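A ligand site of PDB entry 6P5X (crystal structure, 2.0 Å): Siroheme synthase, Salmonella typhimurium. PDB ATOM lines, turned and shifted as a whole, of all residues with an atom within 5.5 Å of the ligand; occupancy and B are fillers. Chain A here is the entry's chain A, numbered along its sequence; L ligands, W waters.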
ATOM      1  N   PRO A 225       2.472  32.319 -23.389  1.00  0.00           N
ATOM      2  CA  PRO A 225       2.975  30.943 -23.356  1.00  0.00           C
ATOM      3  C   PRO A 225       2.041  29.908 -23.974  1.00  0.00           C
ATOM      4  O   PRO A 225       2.458  28.751 -24.139  1.00  0.00           O
ATOM      5  CB  PRO A 225       3.202  30.664 -21.865  1.00  0.00           C
ATOM      6  CG  PRO A 225       2.395  31.691 -21.142  1.00  0.00           C
ATOM      7  CD  PRO A 225       2.047  32.813 -22.069  1.00  0.00           C
ATOM      8  N   GLY A 226       0.821  30.269 -24.351  1.00  0.00           N
ATOM      9  CA  GLY A 226      -0.021  29.303 -25.032  1.00  0.00           C
ATOM     10  C   GLY A 226      -1.517  29.554 -24.892  1.00  0.00           C
ATOM     11  O   GLY A 226      -2.234  29.507 -25.900  1.00  0.00           O
ATOM     12  N   LEU A 250       6.389  27.832 -31.015  1.00  0.00           N
ATOM     13  CA  LEU A 250       5.986  28.154 -29.654  1.00  0.00           C
ATOM     14  C   LEU A 250       4.743  29.042 -29.589  1.00  0.00           C
ATOM     15  O   LEU A 250       4.332  29.417 -28.488  1.00  0.00           O
ATOM     16  CB  LEU A 250       7.146  28.811 -28.909  1.00  0.00           C
ATOM     17  CG  LEU A 250       8.271  27.834 -28.560  1.00  0.00           C
ATOM     18  CD1 LEU A 250       9.480  28.559 -28.015  1.00  0.00           C
ATOM     19  CD2 LEU A 250       7.783  26.784 -27.571  1.00  0.00           C
ATOM     20  N   GLY A 301       6.539  33.278 -29.278  1.00  0.00           N
ATOM     21  CA  GLY A 301       6.116  32.671 -28.027  1.00  0.00           C
ATOM     22  C   GLY A 301       6.527  33.528 -26.834  1.00  0.00           C
ATOM     23  O   GLY A 301       7.607  34.124 -26.813  1.00  0.00           O
ATOM     24  N   GLY A 302       5.656  33.580 -25.826  1.00  0.00           N
ATOM     25  CA  GLY A 302       6.006  34.319 -24.606  1.00  0.00           C
ATOM     26  C   GLY A 302       6.144  35.819 -24.851  1.00  0.00           C
ATOM     27  O   GLY A 302       5.262  36.444 -25.458  1.00  0.00           O
ATOM     28  N   ASP A 303       7.257  36.408 -24.380  1.00  0.00           N
ATOM     29  CA  ASP A 303       7.627  37.819 -24.524  1.00  0.00           C
ATOM     30  C   ASP A 303       8.759  37.990 -25.543  1.00  0.00           C
ATOM     31  O   ASP A 303       9.713  37.208 -25.552  1.00  0.00           O
ATOM     32  CB  ASP A 303       8.067  38.410 -23.175  1.00  0.00           C
ATOM     33  CG  ASP A 303       8.400  39.898 -23.275  1.00  0.00           C
ATOM     34  OD1 ASP A 303       7.480  40.710 -23.511  1.00  0.00           O
ATOM     35  OD2 ASP A 303       9.597  40.252 -23.137  1.00  0.00           O
ATOM     36  N   PRO A 304       8.691  39.003 -26.419  1.00  0.00           N
ATOM     37  CA  PRO A 304       9.674  39.094 -27.526  1.00  0.00           C
ATOM     38  C   PRO A 304      11.093  39.412 -27.076  1.00  0.00           C
ATOM     39  O   PRO A 304      12.041  39.109 -27.811  1.00  0.00           O
ATOM     40  CB  PRO A 304       9.119  40.226 -28.411  1.00  0.00           C
ATOM     41  CG  PRO A 304       7.676  40.370 -27.992  1.00  0.00           C
ATOM     42  CD  PRO A 304       7.661  40.046 -26.520  1.00  0.00           C
ATOM     43  N   ILE A 306      12.621  38.459 -24.064  1.00  0.00           N
ATOM     44  CA  ILE A 306      13.217  37.560 -23.077  1.00  0.00           C
ATOM     45  C   ILE A 306      13.561  36.258 -23.806  1.00  0.00           C
ATOM     46  O   ILE A 306      12.690  35.423 -24.040  1.00  0.00           O
ATOM     47  CB  ILE A 306      12.281  37.291 -21.893  1.00  0.00           C
ATOM     48  CG1 ILE A 306      12.062  38.593 -21.095  1.00  0.00           C
ATOM     49  CG2 ILE A 306      12.864  36.174 -20.999  1.00  0.00           C
ATOM     50  CD1 ILE A 306      10.882  38.522 -20.074  1.00  0.00           C
ATOM     51  N   PHE A 307      14.851  36.085 -24.144  1.00  0.00           N
ATOM     52  CA  PHE A 307      15.365  34.909 -24.855  1.00  0.00           C
ATOM     53  C   PHE A 307      14.591  34.652 -26.150  1.00  0.00           C
ATOM     54  O   PHE A 307      14.435  33.502 -26.570  1.00  0.00           O
ATOM     55  CB  PHE A 307      15.354  33.646 -23.982  1.00  0.00           C
ATOM     56  CG  PHE A 307      16.146  33.782 -22.713  1.00  0.00           C
ATOM     57  CD1 PHE A 307      17.510  34.048 -22.758  1.00  0.00           C
ATOM     58  CD2 PHE A 307      15.527  33.672 -21.468  1.00  0.00           C
ATOM     59  CE1 PHE A 307      18.244  34.195 -21.584  1.00  0.00           C
ATOM     60  CE2 PHE A 307      16.251  33.817 -20.305  1.00  0.00           C
ATOM     61  CZ  PHE A 307      17.606  34.080 -20.359  1.00  0.00           C
ATOM     62  N   GLY A 308      14.127  35.715 -26.799  1.00  0.00           N
ATOM     63  CA  GLY A 308      13.375  35.570 -28.015  1.00  0.00           C
ATOM     64  C   GLY A 308      14.101  36.043 -29.270  1.00  0.00           C
ATOM     65  O   GLY A 308      13.557  35.929 -30.382  1.00  0.00           O
ATOM     66  N   ILE A 330       3.151  37.810 -22.075  1.00  0.00           N
ATOM     67  CA  ILE A 330       3.366  37.061 -20.851  1.00  0.00           C
ATOM     68  C   ILE A 330       4.518  36.074 -21.071  1.00  0.00           C
ATOM     69  O   ILE A 330       4.399  35.157 -21.885  1.00  0.00           O
ATOM     70  CB  ILE A 330       2.084  36.334 -20.419  1.00  0.00           C
ATOM     71  CG1 ILE A 330       0.887  37.315 -20.234  1.00  0.00           C
ATOM     72  CG2 ILE A 330       2.354  35.504 -19.148  1.00  0.00           C
ATOM     73  CD1 ILE A 330       1.067  38.321 -19.126  1.00  0.00           C
ATOM     74  N   THR A 331       5.605  36.248 -20.339  1.00  0.00           N
ATOM     75  CA  THR A 331       6.727  35.334 -20.520  1.00  0.00           C
ATOM     76  C   THR A 331       6.411  33.986 -19.873  1.00  0.00           C
ATOM     77  O   THR A 331       5.508  33.862 -19.038  1.00  0.00           O
ATOM     78  CB  THR A 331       8.031  35.937 -19.974  1.00  0.00           C
ATOM     79  OG1 THR A 331       9.156  35.160 -20.416  1.00  0.00           O
ATOM     80  CG2 THR A 331       8.026  36.014 -18.452  1.00  0.00           C
ATOM     81  N   ALA A 332       7.123  32.950 -20.321  1.00  0.00           N
ATOM     82  CA  ALA A 332       6.863  31.615 -19.797  1.00  0.00           C
ATOM     83  C   ALA A 332       6.941  31.602 -18.273  1.00  0.00           C
ATOM     84  O   ALA A 332       6.117  30.955 -17.628  1.00  0.00           O
ATOM     85  CB  ALA A 332       7.869  30.625 -20.382  1.00  0.00           C
ATOM     86  N   ALA A 333       7.929  32.293 -17.710  1.00  0.00           N
ATOM     87  CA  ALA A 333       8.081  32.337 -16.247  1.00  0.00           C
ATOM     88  C   ALA A 333       6.802  32.798 -15.556  1.00  0.00           C
ATOM     89  O   ALA A 333       6.304  32.148 -14.626  1.00  0.00           O
ATOM     90  CB  ALA A 333       9.249  33.240 -15.872  1.00  0.00           C
ATOM     91  N   CYS A 336       3.741  30.187 -16.342  1.00  0.00           N
ATOM     92  CA  CYS A 336       3.920  28.898 -15.659  1.00  0.00           C
ATOM     93  C   CYS A 336       3.792  29.033 -14.154  1.00  0.00           C
ATOM     94  O   CYS A 336       3.196  28.172 -13.493  1.00  0.00           O
ATOM     95  CB  CYS A 336       5.277  28.311 -16.028  1.00  0.00           C
ATOM     96  SG  CYS A 336       5.298  27.696 -17.708  1.00  0.00           S
ATOM     97  N   PHE A 380      14.793  28.248 -15.247  1.00  0.00           N
ATOM     98  CA  PHE A 380      15.592  27.902 -16.411  1.00  0.00           C
ATOM     99  C   PHE A 380      14.691  27.740 -17.631  1.00  0.00           C
ATOM    100  O   PHE A 380      13.759  26.915 -17.608  1.00  0.00           O
ATOM    101  CB  PHE A 380      16.402  26.630 -16.178  1.00  0.00           C
ATOM    102  CG  PHE A 380      17.433  26.755 -15.098  1.00  0.00           C
ATOM    103  CD1 PHE A 380      17.102  26.508 -13.773  1.00  0.00           C
ATOM    104  CD2 PHE A 380      18.742  27.108 -15.396  1.00  0.00           C
ATOM    105  CE1 PHE A 380      18.063  26.614 -12.751  1.00  0.00           C
ATOM    106  CE2 PHE A 380      19.718  27.207 -14.386  1.00  0.00           C
ATOM    107  CZ  PHE A 380      19.370  26.961 -13.065  1.00  0.00           C
ATOM    108  N   TYR A 381      14.991  28.509 -18.671  1.00  0.00           N
ATOM    109  CA  TYR A 381      14.437  28.337 -20.015  1.00  0.00           C
ATOM    110  C   TYR A 381      15.357  27.434 -20.824  1.00  0.00           C
ATOM    111  O   TYR A 381      16.584  27.526 -20.700  1.00  0.00           O
ATOM    112  CB  TYR A 381      14.336  29.683 -20.736  1.00  0.00           C
ATOM    113  CG  TYR A 381      13.294  30.659 -20.222  1.00  0.00           C
ATOM    114  CD1 TYR A 381      13.339  31.157 -18.917  1.00  0.00           C
ATOM    115  CD2 TYR A 381      12.292  31.132 -21.073  1.00  0.00           C
ATOM    116  CE1 TYR A 381      12.360  32.089 -18.452  1.00  0.00           C
ATOM    117  CE2 TYR A 381      11.327  32.057 -20.619  1.00  0.00           C
ATOM    118  CZ  TYR A 381      11.366  32.523 -19.320  1.00  0.00           C
ATOM    119  OH  TYR A 381      10.410  33.441 -18.902  1.00  0.00           O
ATOM    120  N   MET A 382      14.766  26.588 -21.687  1.00  0.00           N
ATOM    121  CA  MET A 382      15.522  25.750 -22.634  1.00  0.00           C
ATOM    122  C   MET A 382      16.555  24.881 -21.904  1.00  0.00           C
ATOM    123  O   MET A 382      17.681  24.706 -22.374  1.00  0.00           O
ATOM    124  CB  MET A 382      16.239  26.580 -23.703  1.00  0.00           C
ATOM    125  CG  MET A 382      15.371  27.368 -24.674  1.00  0.00           C
ATOM    126  SD  MET A 382      16.381  28.499 -25.676  1.00  0.00           S
ATOM    127  CE  MET A 382      16.907  29.662 -24.418  1.00  0.00           C
ATOM    128  N   GLY A 383      16.162  24.338 -20.754  1.00  0.00           N
ATOM    129  CA  GLY A 383      17.141  23.652 -19.909  1.00  0.00           C
ATOM    130  C   GLY A 383      16.932  22.168 -19.710  1.00  0.00           C
ATOM    131  O   GLY A 383      17.664  21.548 -18.937  1.00  0.00           O
ATOM    132  N   VAL A 408       7.414  22.546 -15.401  1.00  0.00           N
ATOM    133  CA  VAL A 408       6.100  22.826 -15.985  1.00  0.00           C
ATOM    134  C   VAL A 408       6.199  22.597 -17.488  1.00  0.00           C
ATOM    135  O   VAL A 408       6.935  23.304 -18.192  1.00  0.00           O
ATOM    136  CB  VAL A 408       5.634  24.258 -15.684  1.00  0.00           C
ATOM    137  CG1 VAL A 408       4.202  24.446 -16.156  1.00  0.00           C
ATOM    138  CG2 VAL A 408       5.748  24.568 -14.202  1.00  0.00           C
ATOM    139  N   GLU A 409       5.449  21.614 -17.976  1.00  0.00           N
ATOM    140  CA  GLU A 409       5.437  21.266 -19.377  1.00  0.00           C
ATOM    141  C   GLU A 409       4.184  21.836 -20.038  1.00  0.00           C
ATOM    142  O   GLU A 409       3.080  21.623 -19.533  1.00  0.00           O
ATOM    143  CB  GLU A 409       5.463  19.742 -19.542  1.00  0.00           C
ATOM    144  CG  GLU A 409       5.279  19.254 -20.956  1.00  0.00           C
ATOM    145  CD  GLU A 409       5.167  17.736 -21.024  1.00  0.00           C
ATOM    146  OE1 GLU A 409       4.107  17.198 -20.648  1.00  0.00           O
ATOM    147  OE2 GLU A 409       6.135  17.096 -21.452  1.00  0.00           O
ATOM    148  N   ASN A 410       4.350  22.536 -21.152  1.00  0.00           N
ATOM    149  CA  ASN A 410       3.228  23.162 -21.851  1.00  0.00           C
ATOM    150  C   ASN A 410       2.409  24.016 -20.889  1.00  0.00           C
ATOM    151  O   ASN A 410       1.182  23.881 -20.768  1.00  0.00           O
ATOM    152  CB  ASN A 410       2.344  22.129 -22.544  1.00  0.00           C
ATOM    153  CG  ASN A 410       2.968  21.569 -23.798  1.00  0.00           C
ATOM    154  OD1 ASN A 410       3.443  22.317 -24.662  1.00  0.00           O
ATOM    155  ND2 ASN A 410       2.967  20.247 -23.928  1.00  0.00           N
ATOM    156  N   GLY A 411       3.098  24.908 -20.186  1.00  0.00           N
ATOM    157  CA  GLY A 411       2.450  25.754 -19.194  1.00  0.00           C
ATOM    158  C   GLY A 411       1.332  26.589 -19.790  1.00  0.00           C
ATOM    159  O   GLY A 411       1.458  27.111 -20.902  1.00  0.00           O
ATOM    160  N   THR A 412       0.233  26.715 -19.038  1.00  0.00           N
ATOM    161  CA  THR A 412      -1.001  27.433 -19.371  1.00  0.00           C
ATOM    162  C   THR A 412      -1.846  26.753 -20.441  1.00  0.00           C
ATOM    163  O   THR A 412      -2.994  27.177 -20.665  1.00  0.00           O
ATOM    164  CB  THR A 412      -0.745  28.895 -19.804  1.00  0.00           C
ATOM    165  OG1 THR A 412      -0.388  28.967 -21.198  1.00  0.00           O
ATOM    166  CG2 THR A 412       0.321  29.593 -18.894  1.00  0.00           C
ATOM    167  N   PRO A 436       7.854  22.029 -24.838  1.00  0.00           N
ATOM    168  CA  PRO A 436       8.519  23.086 -24.074  1.00  0.00           C
ATOM    169  C   PRO A 436       8.314  22.941 -22.569  1.00  0.00           C
ATOM    170  O   PRO A 436       7.172  22.761 -22.115  1.00  0.00           O
ATOM    171  CB  PRO A 436       7.830  24.350 -24.593  1.00  0.00           C
ATOM    172  CG  PRO A 436       6.430  23.900 -24.960  1.00  0.00           C
ATOM    173  CD  PRO A 436       6.593  22.480 -25.472  1.00  0.00           C
ATOM    174  N   ALA A 437       9.381  23.075 -21.788  1.00  0.00           N
ATOM    175  CA  ALA A 437       9.241  22.943 -20.345  1.00  0.00           C
ATOM    176  C   ALA A 437      10.133  23.941 -19.640  1.00  0.00           C
ATOM    177  O   ALA A 437      11.192  24.340 -20.139  1.00  0.00           O
ATOM    178  CB  ALA A 437       9.565  21.506 -19.888  1.00  0.00           C
ATOM    179  N   LEU A 438       9.676  24.384 -18.483  1.00  0.00           N
ATOM    180  CA  LEU A 438      10.375  25.319 -17.624  1.00  0.00           C
ATOM    181  C   LEU A 438      10.809  24.579 -16.370  1.00  0.00           C
ATOM    182  O   LEU A 438      10.092  23.706 -15.868  1.00  0.00           O
ATOM    183  CB  LEU A 438       9.456  26.489 -17.272  1.00  0.00           C
ATOM    184  CG  LEU A 438       9.991  27.894 -17.108  1.00  0.00           C
ATOM    185  CD1 LEU A 438      10.631  28.401 -18.389  1.00  0.00           C
ATOM    186  CD2 LEU A 438       8.829  28.794 -16.681  1.00  0.00           C
HETATM  187  N1  LIG L   1      10.434  34.337 -25.429  1.00  0.00           N
HETATM  188  C1  LIG L   1       9.839  33.205 -24.694  1.00  0.00           C
HETATM  189  C2  LIG L   1      10.881  32.111 -24.464  1.00  0.00           C
HETATM  190  C3  LIG L   1      11.586  31.606 -25.718  1.00  0.00           C
HETATM  191  S1  LIG L   1      12.966  30.494 -25.298  1.00  0.00           S
HETATM  192  C4  LIG L   1       9.228  33.619 -23.338  1.00  0.00           C
HETATM  193  O1  LIG L   1       9.238  34.785 -22.955  1.00  0.00           O
HETATM  194  O2  LIG L   1       8.739  32.787 -22.578  1.00  0.00           O
HETATM  195  C5  LIG L   1      11.987  28.971 -25.316  1.00  0.00           C
HETATM  196  C6  LIG L   1      11.803  28.348 -23.930  1.00  0.00           C
HETATM  197  O3  LIG L   1      10.708  28.953 -23.230  1.00  0.00           O
HETATM  198  C7  LIG L   1      11.446  26.873 -23.968  1.00  0.00           C
HETATM  199  O4  LIG L   1      12.586  26.059 -24.102  1.00  0.00           O
HETATM  200  C8  LIG L   1      10.806  26.653 -22.618  1.00  0.00           C
HETATM  201  O5  LIG L   1      11.828  26.495 -21.638  1.00  0.00           O
HETATM  202  C9  LIG L   1      10.137  27.992 -22.362  1.00  0.00           C
HETATM  203  N2  LIG L   1       8.691  27.948 -22.648  1.00  0.00           N
HETATM  204  C10 LIG L   1       8.026  28.608 -23.649  1.00  0.00           C
HETATM  205  N3  LIG L   1       6.707  28.306 -23.560  1.00  0.00           N
HETATM  206  C11 LIG L   1       6.534  27.456 -22.520  1.00  0.00           C
HETATM  207  C12 LIG L   1       5.415  26.830 -21.980  1.00  0.00           C
HETATM  208  N4  LIG L   1       4.179  27.009 -22.475  1.00  0.00           N
HETATM  209  N5  LIG L   1       5.588  26.014 -20.887  1.00  0.00           N
HETATM  210  C13 LIG L   1       6.823  25.789 -20.332  1.00  0.00           C
HETATM  211  N6  LIG L   1       7.925  26.417 -20.876  1.00  0.00           N
HETATM  212  C14 LIG L   1       7.775  27.231 -21.941  1.00  0.00           C
HETATM  213  O   HOH W   1      12.208  25.098 -26.680  1.00  0.00           O
HETATM  214  O   HOH W   2      10.102  33.922 -28.083  1.00  0.00           O
HETATM  215  O   HOH W   3       5.519  29.882 -25.874  1.00  0.00           O
HETATM  216  O   HOH W   4       8.270  30.691 -26.148  1.00  0.00           O
HETATM  217  O   HOH W   5      11.937  23.241 -23.331  1.00  0.00           O
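Water W2 lies within hydrogen-bond range of a nitrogen (N1) of the ligand and the backbone carbonyl oxygen (O) of Gly 301.
Water W5 bridges the backbone NH of Ala 437 and an oxygen (O4) of the ligand.
Water W3 lies within hydrogen-bond range of the backbone carbonyl oxygen (O) of Leu 250 (2.9 Å) and a nitrogen (N3) of the ligand (3.0 Å).
N1 of the ligand is in hydrogen-bond range of O of Gly 301, at 3.2 Å.
SG of Cys 336 lies close to N5 of the ligand (3.6 Å).
A nitrogen (N1) of the ligand is in hydrogen-bond range of the backbone carbonyl oxygen (O) of Ile 306 (2.9 Å).
An oxygen (O2) of the ligand lies within hydrogen-bond range of the backbone NH (N) of Ala 332 (2.8 Å).
O of Ala 437 sits at hydrogen-bond distance from O5 of the ligand, 2.7 Å away.
OG1 of Thr 331 is in hydrogen-bond range of O1 of the ligand (2.6 Å).
N of Asp 303 is in hydrogen-bond range of O1 of the ligand (2.9 Å).
N1 of the ligand lies within hydrogen-bond range of O of Asp 303, at 3.0 Å.
The backbone NH (N) of Gly 411 sits at hydrogen-bond distance from a nitrogen (N5) of the ligand (2.8 Å).
An oxygen (O5) of the ligand is in hydrogen-bond range of the backbone NH (N) of Met 382 (2.9 Å).
The backbone carbonyl oxygen (O) of Pro 225 lies within hydrogen-bond range of a nitrogen (N4) of the ligand.
The backbone carbonyl oxygen (O) of Gly 411 lies within hydrogen-bond range of a nitrogen (N4) of the ligand, at 3.1 Å.
O of Phe 307 lies close to S1 of the ligand.
Leu 250 touches the ligand.
Gly 302 touches the ligand (CA to C4, 3.5 Å).
Tyr 381 touches the ligand (CE2 to O2, 3.3 Å).
Val 408 touches the ligand.
Asn 410 touches the ligand (N to N5, 3.7 Å).
Pro 436 touches the ligand.
N of Leu 438 touches N6 of the ligand, 3.6 Å away.
Within 4 Å of the ligand: Pro 225, Leu 250, Gly 301, Gly 302, Asp 303, Ile 306, Phe 307, Thr 331, Ala 332, Cys 336, Tyr 381, Met 382, Val 408, Asn 410, Gly 411, Pro 436, Ala 437 and Leu 438.
The nearest printed residue that does not touch the ligand is Gly 308 (4.1 Å).
N of Val 408 lies within hydrogen-bond range of O of Leu 438.
O of Ala 332 lies close to SG of Cys 336 (3.4 Å).
The backbone NH (N) of Ala 333 lies within hydrogen-bond range of the side-chain hydroxyl (OH) of Tyr 381 (3.0 Å).
The backbone carbonyl oxygen (O) of Pro 436 sits at hydrogen-bond distance from the backbone NH (N) of Asn 410.
OG1 of Thr 331 lies within hydrogen-bond range of OH of Tyr 381, at 2.6 Å.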
